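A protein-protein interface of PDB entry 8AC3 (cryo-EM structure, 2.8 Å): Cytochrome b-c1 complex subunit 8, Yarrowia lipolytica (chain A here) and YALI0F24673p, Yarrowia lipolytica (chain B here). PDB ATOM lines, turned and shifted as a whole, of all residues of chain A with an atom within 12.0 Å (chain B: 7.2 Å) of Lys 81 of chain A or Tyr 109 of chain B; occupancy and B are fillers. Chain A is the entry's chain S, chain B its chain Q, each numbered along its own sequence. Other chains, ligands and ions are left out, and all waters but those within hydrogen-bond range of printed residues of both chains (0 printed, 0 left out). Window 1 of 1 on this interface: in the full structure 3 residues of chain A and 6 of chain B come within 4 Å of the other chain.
NZ of Lys 81 of chain A lies within hydrogen-bond range of SG of Cys 91 of chain B.
NZ of Lys 81 of chain A lies within salt-bridge range of OE1 of Glu 111 of chain B, at 2.8 Å.
O of Asp 112 of chain B is in hydrogen-bond range of NZ of Lys 81 of chain A, at 2.8 Å.
OE2 of Glu 115 of chain B is in hydrogen-bond range of N of Lys 81 of chain A, at 2.8 Å.
The side-chain amino group (NZ) of Lys 81 of chain A lies within salt-bridge range of the side-chain carboxylate (OE2) of Glu 116 of chain B, 2.7 Å away.
The guanidinium group (NH2) of Arg 94 of chain B sits close to the side-chain sulfur (SG) of Cys 91 of chain B, 3.7 Å away.
The side-chain sulfur of Cys 113 of chain B is disulfide-bonded to the side-chain sulfur of Cys 91 of chain B, at 2.1 Å.
NH1 of Arg 94 of chain B lies within salt-bridge range of OE2 of Glu 111 of chain B, 3.1 Å away.
N of Val 114 of chain B is in hydrogen-bond range of OD1 of Asp 112 of chain B (3.0 Å).
The side-chain hydroxyl of Thr 80 of chain A lies within hydrogen-bond range of the backbone carbonyl oxygen of Trp 77 of chain A (2.7 Å).
Among the printed residues, merely in contact across the chains: Thr 80 of chain A with Glu 115 of chain B, Lys 81 of chain A with Tyr 109 of chain B and Arg 84 of chain A with Tyr 109 of chain B.
Lys 81 of chain A touches six residues of chain B.
Tyr 109 of chain B touches two residues of chain A.
Cys 91 of chain B touches just one residue of chain A: Lys 81.
Glu 111 of chain B touches just one residue of chain A: Lys 81 (2.8 Å).
Asp 112 of chain B touches just one residue of chain A: Lys 81.
Cys 113 of chain B touches none of the printed residues of chain A.
No residue of chain A comes within 4 Å of Val 114 of chain B.
Printed residues of chain B within 4 Å of Thr 80 of chain A: Glu 115 (3.3 Å).
Printed residues of chain A within 4 Å of Glu 116 of chain B: Lys 81 (2.7 Å).
Of the printed residues of chain B, Arg 84 of chain A touches Tyr 109.
His 85 of chain A touches none of the printed residues of chain B.
Val 95 of chain B touches none of the printed residues of chain A.
The nearest residue of chain B that does not touch Lys 81 of chain A is Cys 113 of chain B (4.2 Å).
The nearest residue of chain A that does not touch Tyr 109 of chain B is Ala 82 of chain A (6.7 Å).
The nearest printed residue of chain B that does not touch Thr 80 of chain A is Tyr 109 of chain B (6.9 Å).
Of the 17 printed residues of chain A, 3 touch a printed residue of chain B.
Printed residues of chain A that touch a printed residue of chain B: Thr 80, Lys 81 and Arg 84.
Along chain B the printed residues that touch a printed residue of chain A span positions 91 to 116.
Among the printed residues, 8 pairs touch across the chains.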
ATOM      1  N   GLU A  73      12.384   7.139   8.855  1.00  0.00           N
ATOM      2  CA  GLU A  73      11.919   7.800  10.067  1.00  0.00           C
ATOM      3  C   GLU A  73      10.666   7.128  10.616  1.00  0.00           C
ATOM      4  O   GLU A  73      10.477   7.073  11.832  1.00  0.00           O
ATOM      5  CB  GLU A  73      11.640   9.277   9.828  1.00  0.00           C
ATOM      6  CG  GLU A  73      12.884  10.134   9.958  1.00  0.00           C
ATOM      7  CD  GLU A  73      12.927  11.382   9.090  1.00  0.00           C
ATOM      8  OE1 GLU A  73      11.865  11.785   8.559  1.00  0.00           O
ATOM      9  OE2 GLU A  73      14.031  11.957   8.948  1.00  0.00           O
ATOM     10  N   LYS A  74       9.798   6.649   9.718  1.00  0.00           N
ATOM     11  CA  LYS A  74       8.595   5.967  10.163  1.00  0.00           C
ATOM     12  C   LYS A  74       8.993   4.653  10.815  1.00  0.00           C
ATOM     13  O   LYS A  74       8.439   4.274  11.840  1.00  0.00           O
ATOM     14  CB  LYS A  74       7.660   5.622   9.000  1.00  0.00           C
ATOM     15  CG  LYS A  74       6.291   5.099   9.415  1.00  0.00           C
ATOM     16  CD  LYS A  74       5.414   6.165  10.061  1.00  0.00           C
ATOM     17  CE  LYS A  74       4.011   5.703  10.406  1.00  0.00           C
ATOM     18  NZ  LYS A  74       3.056   5.937   9.296  1.00  0.00           N
ATOM     19  N   ASN A  75       9.941   3.961  10.173  1.00  0.00           N
ATOM     20  CA  ASN A  75      10.322   2.646  10.638  1.00  0.00           C
ATOM     21  C   ASN A  75      10.889   2.801  12.038  1.00  0.00           C
ATOM     22  O   ASN A  75      10.575   1.997  12.906  1.00  0.00           O
ATOM     23  CB  ASN A  75      11.308   1.946   9.706  1.00  0.00           C
ATOM     24  CG  ASN A  75      11.930   0.716  10.335  1.00  0.00           C
ATOM     25  OD1 ASN A  75      13.011   0.795  10.917  1.00  0.00           O
ATOM     26  ND2 ASN A  75      11.261  -0.421  10.229  1.00  0.00           N
ATOM     27  N   GLU A  76      11.679   3.863  12.236  1.00  0.00           N
ATOM     28  CA  GLU A  76      12.317   4.085  13.522  1.00  0.00           C
ATOM     29  C   GLU A  76      11.242   4.310  14.579  1.00  0.00           C
ATOM     30  O   GLU A  76      11.348   3.796  15.689  1.00  0.00           O
ATOM     31  CB  GLU A  76      13.314   5.245  13.457  1.00  0.00           C
ATOM     32  CG  GLU A  76      13.735   5.791  14.816  1.00  0.00           C
ATOM     33  CD  GLU A  76      14.918   6.751  14.836  1.00  0.00           C
ATOM     34  OE1 GLU A  76      15.740   6.711  13.891  1.00  0.00           O
ATOM     35  OE2 GLU A  76      15.025   7.539  15.807  1.00  0.00           O
ATOM     36  N   TRP A  77      10.218   5.075  14.203  1.00  0.00           N
ATOM     37  CA  TRP A  77       9.185   5.483  15.132  1.00  0.00           C
ATOM     38  C   TRP A  77       8.272   4.312  15.485  1.00  0.00           C
ATOM     39  O   TRP A  77       7.769   4.248  16.601  1.00  0.00           O
ATOM     40  CB  TRP A  77       8.414   6.672  14.561  1.00  0.00           C
ATOM     41  CG  TRP A  77       7.330   7.134  15.477  1.00  0.00           C
ATOM     42  CD1 TRP A  77       7.458   7.973  16.546  1.00  0.00           C
ATOM     43  CD2 TRP A  77       5.947   6.744  15.426  1.00  0.00           C
ATOM     44  NE1 TRP A  77       6.245   8.151  17.155  1.00  0.00           N
ATOM     45  CE2 TRP A  77       5.303   7.405  16.495  1.00  0.00           C
ATOM     46  CE3 TRP A  77       5.197   5.914  14.584  1.00  0.00           C
ATOM     47  CZ2 TRP A  77       3.940   7.256  16.741  1.00  0.00           C
ATOM     48  CZ3 TRP A  77       3.847   5.769  14.824  1.00  0.00           C
ATOM     49  CH2 TRP A  77       3.232   6.439  15.886  1.00  0.00           C
ATOM     50  N   LEU A  78       8.068   3.383  14.546  1.00  0.00           N
ATOM     51  CA  LEU A  78       7.180   2.251  14.779  1.00  0.00           C
ATOM     52  C   LEU A  78       7.760   1.306  15.821  1.00  0.00           C
ATOM     53  O   LEU A  78       7.023   0.546  16.444  1.00  0.00           O
ATOM     54  CB  LEU A  78       7.016   1.474  13.474  1.00  0.00           C
ATOM     55  CG  LEU A  78       6.012   2.069  12.496  1.00  0.00           C
ATOM     56  CD1 LEU A  78       6.024   1.295  11.189  1.00  0.00           C
ATOM     57  CD2 LEU A  78       4.621   2.057  13.101  1.00  0.00           C
ATOM     58  N   TYR A  79       9.090   1.308  15.957  1.00  0.00           N
ATOM     59  CA  TYR A  79       9.748   0.377  16.857  1.00  0.00           C
ATOM     60  C   TYR A  79      10.159   1.092  18.137  1.00  0.00           C
ATOM     61  O   TYR A  79      11.069   0.648  18.835  1.00  0.00           O
ATOM     62  CB  TYR A  79      10.880  -0.346  16.123  1.00  0.00           C
ATOM     63  CG  TYR A  79      10.380  -1.404  15.176  1.00  0.00           C
ATOM     64  CD1 TYR A  79      10.214  -2.715  15.592  1.00  0.00           C
ATOM     65  CD2 TYR A  79       9.998  -1.081  13.881  1.00  0.00           C
ATOM     66  CE1 TYR A  79       9.715  -3.688  14.736  1.00  0.00           C
ATOM     67  CE2 TYR A  79       9.500  -2.039  13.009  1.00  0.00           C
ATOM     68  CZ  TYR A  79       9.354  -3.348  13.440  1.00  0.00           C
ATOM     69  OH  TYR A  79       8.859  -4.295  12.590  1.00  0.00           O
ATOM     70  N   THR A  80       9.499   2.218  18.419  1.00  0.00           N
ATOM     71  CA  THR A  80       9.580   2.835  19.733  1.00  0.00           C
ATOM     72  C   THR A  80       8.352   2.417  20.541  1.00  0.00           C
ATOM     73  O   THR A  80       7.489   1.711  20.022  1.00  0.00           O
ATOM     74  CB  THR A  80       9.786   4.352  19.633  1.00  0.00           C
ATOM     75  OG1 THR A  80       8.635   4.931  19.017  1.00  0.00           O
ATOM     76  CG2 THR A  80      11.034   4.743  18.870  1.00  0.00           C
ATOM     77  N   LYS A  81       8.306   2.848  21.810  1.00  0.00           N
ATOM     78  CA  LYS A  81       7.192   2.639  22.721  1.00  0.00           C
ATOM     79  C   LYS A  81       5.948   3.337  22.184  1.00  0.00           C
ATOM     80  O   LYS A  81       4.846   2.787  22.211  1.00  0.00           O
ATOM     81  CB  LYS A  81       7.496   3.329  24.053  1.00  0.00           C
ATOM     82  CG  LYS A  81       8.035   2.452  25.166  1.00  0.00           C
ATOM     83  CD  LYS A  81       8.349   3.270  26.387  1.00  0.00           C
ATOM     84  CE  LYS A  81       9.571   2.758  27.111  1.00  0.00           C
ATOM     85  NZ  LYS A  81       9.846   3.564  28.320  1.00  0.00           N
ATOM     86  N   ALA A  82       6.156   4.582  21.742  1.00  0.00           N
ATOM     87  CA  ALA A  82       5.126   5.464  21.226  1.00  0.00           C
ATOM     88  C   ALA A  82       4.465   4.856  19.992  1.00  0.00           C
ATOM     89  O   ALA A  82       3.291   5.115  19.729  1.00  0.00           O
ATOM     90  CB  ALA A  82       5.751   6.798  20.912  1.00  0.00           C
ATOM     91  N   GLY A  83       5.223   4.031  19.257  1.00  0.00           N
ATOM     92  CA  GLY A  83       4.770   3.505  17.978  1.00  0.00           C
ATOM     93  C   GLY A  83       4.190   2.096  18.077  1.00  0.00           C
ATOM     94  O   GLY A  83       3.991   1.456  17.042  1.00  0.00           O
ATOM     95  N   ARG A  84       3.921   1.637  19.312  1.00  0.00           N
ATOM     96  CA  ARG A  84       3.525   0.266  19.601  1.00  0.00           C
ATOM     97  C   ARG A  84       2.242  -0.096  18.869  1.00  0.00           C
ATOM     98  O   ARG A  84       2.116  -1.199  18.338  1.00  0.00           O
ATOM     99  CB  ARG A  84       3.122   0.120  21.063  1.00  0.00           C
ATOM    100  CG  ARG A  84       4.227  -0.385  21.972  1.00  0.00           C
ATOM    101  CD  ARG A  84       3.551  -0.802  23.258  1.00  0.00           C
ATOM    102  NE  ARG A  84       2.954   0.311  23.990  1.00  0.00           N
ATOM    103  CZ  ARG A  84       1.777   0.270  24.608  1.00  0.00           C
ATOM    104  NH1 ARG A  84       1.041  -0.830  24.575  1.00  0.00           N
ATOM    105  NH2 ARG A  84       1.333   1.337  25.247  1.00  0.00           N
ATOM    106  N   HIS A  85       1.278   0.827  18.925  1.00  0.00           N
ATOM    107  CA  HIS A  85      -0.069   0.571  18.455  1.00  0.00           C
ATOM    108  C   HIS A  85      -0.089   0.555  16.937  1.00  0.00           C
ATOM    109  O   HIS A  85      -0.772  -0.269  16.329  1.00  0.00           O
ATOM    110  CB  HIS A  85      -1.022   1.652  18.959  1.00  0.00           C
ATOM    111  CG  HIS A  85      -1.076   1.734  20.441  1.00  0.00           C
ATOM    112  ND1 HIS A  85      -1.570   0.707  21.220  1.00  0.00           N
ATOM    113  CD2 HIS A  85      -0.706   2.716  21.288  1.00  0.00           C
ATOM    114  CE1 HIS A  85      -1.504   1.055  22.489  1.00  0.00           C
ATOM    115  NE2 HIS A  85      -0.984   2.287  22.556  1.00  0.00           N
ATOM    116  N   GLU A  86       0.630   1.520  16.350  1.00  0.00           N
ATOM    117  CA  GLU A  86       0.702   1.664  14.908  1.00  0.00           C
ATOM    118  C   GLU A  86       1.473   0.480  14.337  1.00  0.00           C
ATOM    119  O   GLU A  86       1.223   0.084  13.201  1.00  0.00           O
ATOM    120  CB  GLU A  86       1.329   2.999  14.500  1.00  0.00           C
ATOM    121  CG  GLU A  86       0.427   4.207  14.707  1.00  0.00           C
ATOM    122  CD  GLU A  86       0.145   4.642  16.140  1.00  0.00           C
ATOM    123  OE1 GLU A  86       0.998   4.398  17.026  1.00  0.00           O
ATOM    124  OE2 GLU A  86      -0.938   5.220  16.373  1.00  0.00           O
ATOM    125  N   LEU A  87       2.398  -0.077  15.137  1.00  0.00           N
ATOM    126  CA  LEU A  87       3.173  -1.224  14.686  1.00  0.00           C
ATOM    127  C   LEU A  87       2.291  -2.468  14.693  1.00  0.00           C
ATOM    128  O   LEU A  87       2.437  -3.337  13.837  1.00  0.00           O
ATOM    129  CB  LEU A  87       4.417  -1.432  15.557  1.00  0.00           C
ATOM    130  CG  LEU A  87       5.265  -2.660  15.213  1.00  0.00           C
ATOM    131  CD1 LEU A  87       5.876  -2.540  13.824  1.00  0.00           C
ATOM    132  CD2 LEU A  87       6.352  -2.892  16.251  1.00  0.00           C
ATOM    133  N   ALA A  88       1.376  -2.529  15.665  1.00  0.00           N
ATOM    134  CA  ALA A  88       0.534  -3.697  15.855  1.00  0.00           C
ATOM    135  C   ALA A  88      -0.421  -3.836  14.672  1.00  0.00           C
ATOM    136  O   ALA A  88      -0.716  -4.949  14.243  1.00  0.00           O
ATOM    137  CB  ALA A  88      -0.207  -3.580  17.162  1.00  0.00           C
ATOM    138  N   LYS A  89      -0.873  -2.683  14.158  1.00  0.00           N
ATOM    139  CA  LYS A  89      -1.785  -2.591  13.029  1.00  0.00           C
ATOM    140  C   LYS A  89      -1.042  -2.900  11.736  1.00  0.00           C
ATOM    141  O   LYS A  89      -1.591  -3.556  10.850  1.00  0.00           O
ATOM    142  CB  LYS A  89      -2.404  -1.195  12.930  1.00  0.00           C
ATOM    143  CG  LYS A  89      -3.418  -0.868  14.015  1.00  0.00           C
ATOM    144  CD  LYS A  89      -3.868   0.575  14.007  1.00  0.00           C
ATOM    145  CE  LYS A  89      -4.404   1.028  15.349  1.00  0.00           C
ATOM    146  NZ  LYS A  89      -5.010   2.377  15.268  1.00  0.00           N
ATOM    147  N   CYS B  91      10.754   7.856  33.797  1.00  0.00           N
ATOM    148  CA  CYS B  91      10.446   6.504  33.359  1.00  0.00           C
ATOM    149  C   CYS B  91      10.592   5.523  34.522  1.00  0.00           C
ATOM    150  O   CYS B  91       9.661   4.750  34.771  1.00  0.00           O
ATOM    151  CB  CYS B  91      11.303   6.057  32.178  1.00  0.00           C
ATOM    152  SG  CYS B  91      10.919   4.397  31.551  1.00  0.00           S
ATOM    153  N   ARG B  94       7.789   5.611  37.012  1.00  0.00           N
ATOM    154  CA  ARG B  94       6.556   5.026  36.492  1.00  0.00           C
ATOM    155  C   ARG B  94       6.616   3.503  36.547  1.00  0.00           C
ATOM    156  O   ARG B  94       5.648   2.864  36.956  1.00  0.00           O
ATOM    157  CB  ARG B  94       6.242   5.474  35.060  1.00  0.00           C
ATOM    158  CG  ARG B  94       5.920   6.957  34.939  1.00  0.00           C
ATOM    159  CD  ARG B  94       5.783   7.556  33.551  1.00  0.00           C
ATOM    160  NE  ARG B  94       6.925   7.382  32.655  1.00  0.00           N
ATOM    161  CZ  ARG B  94       6.897   6.659  31.539  1.00  0.00           C
ATOM    162  NH1 ARG B  94       5.774   6.056  31.183  1.00  0.00           N
ATOM    163  NH2 ARG B  94       7.979   6.562  30.787  1.00  0.00           N
ATOM    164  N   VAL B  95       7.754   2.938  36.129  1.00  0.00           N
ATOM    165  CA  VAL B  95       7.857   1.497  35.965  1.00  0.00           C
ATOM    166  C   VAL B  95       7.876   0.826  37.336  1.00  0.00           C
ATOM    167  O   VAL B  95       7.171  -0.160  37.536  1.00  0.00           O
ATOM    168  CB  VAL B  95       9.032   1.087  35.054  1.00  0.00           C
ATOM    169  CG1 VAL B  95       9.300  -0.408  35.101  1.00  0.00           C
ATOM    170  CG2 VAL B  95       8.787   1.515  33.612  1.00  0.00           C
ATOM    171  N   TYR B 104       0.423  -7.125  38.182  1.00  0.00           N
ATOM    172  CA  TYR B 104       1.354  -6.624  37.185  1.00  0.00           C
ATOM    173  C   TYR B 104       1.916  -7.798  36.386  1.00  0.00           C
ATOM    174  O   TYR B 104       2.180  -7.658  35.193  1.00  0.00           O
ATOM    175  CB  TYR B 104       2.451  -5.773  37.837  1.00  0.00           C
ATOM    176  CG  TYR B 104       3.667  -5.546  36.970  1.00  0.00           C
ATOM    177  CD1 TYR B 104       3.675  -4.571  35.982  1.00  0.00           C
ATOM    178  CD2 TYR B 104       4.801  -6.338  37.104  1.00  0.00           C
ATOM    179  CE1 TYR B 104       4.782  -4.374  35.166  1.00  0.00           C
ATOM    180  CE2 TYR B 104       5.910  -6.165  36.289  1.00  0.00           C
ATOM    181  CZ  TYR B 104       5.905  -5.173  35.320  1.00  0.00           C
ATOM    182  OH  TYR B 104       7.003  -4.988  34.528  1.00  0.00           O
ATOM    183  N   HIS B 106       0.391 -10.486  35.594  1.00  0.00           N
ATOM    184  CA  HIS B 106      -0.645 -10.922  34.666  1.00  0.00           C
ATOM    185  C   HIS B 106      -1.152  -9.736  33.848  1.00  0.00           C
ATOM    186  O   HIS B 106      -2.357  -9.589  33.640  1.00  0.00           O
ATOM    187  CB  HIS B 106      -1.772 -11.671  35.402  1.00  0.00           C
ATOM    188  CG  HIS B 106      -1.330 -12.938  36.058  1.00  0.00           C
ATOM    189  ND1 HIS B 106      -0.988 -14.069  35.337  1.00  0.00           N
ATOM    190  CD2 HIS B 106      -1.159 -13.256  37.360  1.00  0.00           C
ATOM    191  CE1 HIS B 106      -0.629 -15.028  36.169  1.00  0.00           C
ATOM    192  NE2 HIS B 106      -0.726 -14.554  37.417  1.00  0.00           N
ATOM    193  N   ALA B 107      -0.221  -8.887  33.397  1.00  0.00           N
ATOM    194  CA  ALA B 107      -0.550  -7.794  32.495  1.00  0.00           C
ATOM    195  C   ALA B 107      -0.038  -8.123  31.094  1.00  0.00           C
ATOM    196  O   ALA B 107       0.844  -8.970  30.931  1.00  0.00           O
ATOM    197  CB  ALA B 107      -0.024  -6.475  33.018  1.00  0.00           C
ATOM    198  N   GLU B 108      -0.629  -7.461  30.095  1.00  0.00           N
ATOM    199  CA  GLU B 108      -0.297  -7.711  28.704  1.00  0.00           C
ATOM    200  C   GLU B 108       1.035  -7.034  28.377  1.00  0.00           C
ATOM    201  O   GLU B 108       1.970  -7.696  27.916  1.00  0.00           O
ATOM    202  CB  GLU B 108      -1.466  -7.292  27.803  1.00  0.00           C
ATOM    203  CG  GLU B 108      -1.396  -7.855  26.386  1.00  0.00           C
ATOM    204  CD  GLU B 108      -0.471  -7.130  25.419  1.00  0.00           C
ATOM    205  OE1 GLU B 108       0.435  -7.788  24.856  1.00  0.00           O
ATOM    206  OE2 GLU B 108      -0.661  -5.913  25.218  1.00  0.00           O
ATOM    207  N   TYR B 109       1.108  -5.721  28.645  1.00  0.00           N
ATOM    208  CA  TYR B 109       2.271  -4.911  28.315  1.00  0.00           C
ATOM    209  C   TYR B 109       3.012  -4.491  29.583  1.00  0.00           C
ATOM    210  O   TYR B 109       2.473  -3.755  30.406  1.00  0.00           O
ATOM    211  CB  TYR B 109       1.884  -3.697  27.461  1.00  0.00           C
ATOM    212  CG  TYR B 109       3.014  -2.728  27.213  1.00  0.00           C
ATOM    213  CD1 TYR B 109       4.136  -3.104  26.480  1.00  0.00           C
ATOM    214  CD2 TYR B 109       2.978  -1.437  27.725  1.00  0.00           C
ATOM    215  CE1 TYR B 109       5.182  -2.220  26.253  1.00  0.00           C
ATOM    216  CE2 TYR B 109       4.016  -0.541  27.504  1.00  0.00           C
ATOM    217  CZ  TYR B 109       5.122  -0.933  26.765  1.00  0.00           C
ATOM    218  OH  TYR B 109       6.152  -0.062  26.541  1.00  0.00           O
ATOM    219  N   LYS B 110       4.268  -4.939  29.699  1.00  0.00           N
ATOM    220  CA  LYS B 110       5.166  -4.491  30.751  1.00  0.00           C
ATOM    221  C   LYS B 110       6.187  -3.514  30.167  1.00  0.00           C
ATOM    222  O   LYS B 110       7.009  -3.884  29.327  1.00  0.00           O
ATOM    223  CB  LYS B 110       5.835  -5.696  31.415  1.00  0.00           C
ATOM    224  CG  LYS B 110       4.888  -6.691  32.079  1.00  0.00           C
ATOM    225  CD  LYS B 110       5.612  -7.953  32.515  1.00  0.00           C
ATOM    226  CE  LYS B 110       4.768  -8.927  33.311  1.00  0.00           C
ATOM    227  NZ  LYS B 110       3.580  -9.401  32.563  1.00  0.00           N
ATOM    228  N   GLU B 111       6.105  -2.257  30.615  1.00  0.00           N
ATOM    229  CA  GLU B 111       6.987  -1.189  30.166  1.00  0.00           C
ATOM    230  C   GLU B 111       8.386  -1.388  30.753  1.00  0.00           C
ATOM    231  O   GLU B 111       8.517  -1.736  31.926  1.00  0.00           O
ATOM    232  CB  GLU B 111       6.407   0.158  30.599  1.00  0.00           C
ATOM    233  CG  GLU B 111       6.900   1.315  29.755  1.00  0.00           C
ATOM    234  CD  GLU B 111       6.722   2.731  30.273  1.00  0.00           C
ATOM    235  OE1 GLU B 111       7.467   3.597  29.792  1.00  0.00           O
ATOM    236  OE2 GLU B 111       5.841   2.974  31.130  1.00  0.00           O
ATOM    237  N   ASP B 112       9.428  -1.141  29.934  1.00  0.00           N
ATOM    238  CA  ASP B 112      10.798  -1.002  30.410  1.00  0.00           C
ATOM    239  C   ASP B 112      11.259   0.453  30.290  1.00  0.00           C
ATOM    240  O   ASP B 112      10.502   1.321  29.862  1.00  0.00           O
ATOM    241  CB  ASP B 112      11.740  -1.955  29.672  1.00  0.00           C
ATOM    242  CG  ASP B 112      11.691  -1.785  28.162  1.00  0.00           C
ATOM    243  OD1 ASP B 112      12.391  -0.889  27.636  1.00  0.00           O
ATOM    244  OD2 ASP B 112      10.909  -2.520  27.530  1.00  0.00           O
ATOM    245  N   CYS B 113      12.527   0.695  30.637  1.00  0.00           N
ATOM    246  CA  CYS B 113      13.093   2.023  30.511  1.00  0.00           C
ATOM    247  C   CYS B 113      14.333   2.009  29.635  1.00  0.00           C
ATOM    248  O   CYS B 113      15.151   2.928  29.701  1.00  0.00           O
ATOM    249  CB  CYS B 113      13.415   2.584  31.885  1.00  0.00           C
ATOM    250  SG  CYS B 113      11.891   3.030  32.747  1.00  0.00           S
ATOM    251  N   VAL B 114      14.413   0.985  28.788  1.00  0.00           N
ATOM    252  CA  VAL B 114      15.603   0.787  27.986  1.00  0.00           C
ATOM    253  C   VAL B 114      15.740   1.937  26.997  1.00  0.00           C
ATOM    254  O   VAL B 114      16.832   2.471  26.828  1.00  0.00           O
ATOM    255  CB  VAL B 114      15.587  -0.590  27.305  1.00  0.00           C
ATOM    256  CG1 VAL B 114      16.595  -0.693  26.180  1.00  0.00           C
ATOM    257  CG2 VAL B 114      15.837  -1.673  28.323  1.00  0.00           C
ATOM    258  N   GLU B 115      14.617   2.340  26.397  1.00  0.00           N
ATOM    259  CA  GLU B 115      14.636   3.391  25.395  1.00  0.00           C
ATOM    260  C   GLU B 115      15.268   4.660  25.960  1.00  0.00           C
ATOM    261  O   GLU B 115      16.163   5.243  25.348  1.00  0.00           O
ATOM    262  CB  GLU B 115      13.228   3.676  24.888  1.00  0.00           C
ATOM    263  CG  GLU B 115      12.986   3.143  23.493  1.00  0.00           C
ATOM    264  CD  GLU B 115      11.560   3.306  22.996  1.00  0.00           C
ATOM    265  OE1 GLU B 115      11.107   4.463  22.851  1.00  0.00           O
ATOM    266  OE2 GLU B 115      10.897   2.272  22.760  1.00  0.00           O
ATOM    267  N   GLU B 116      14.789   5.057  27.141  1.00  0.00           N
ATOM    268  CA  GLU B 116      15.200   6.293  27.783  1.00  0.00           C
ATOM    269  C   GLU B 116      16.647   6.172  28.230  1.00  0.00           C
ATOM    270  O   GLU B 116      17.398   7.147  28.207  1.00  0.00           O
ATOM    271  CB  GLU B 116      14.310   6.580  28.990  1.00  0.00           C
ATOM    272  CG  GLU B 116      12.974   7.172  28.600  1.00  0.00           C
ATOM    273  CD  GLU B 116      11.913   6.160  28.195  1.00  0.00           C
ATOM    274  OE1 GLU B 116      10.833   6.590  27.759  1.00  0.00           O
ATOM    275  OE2 GLU B 116      12.202   4.949  28.263  1.00  0.00           O
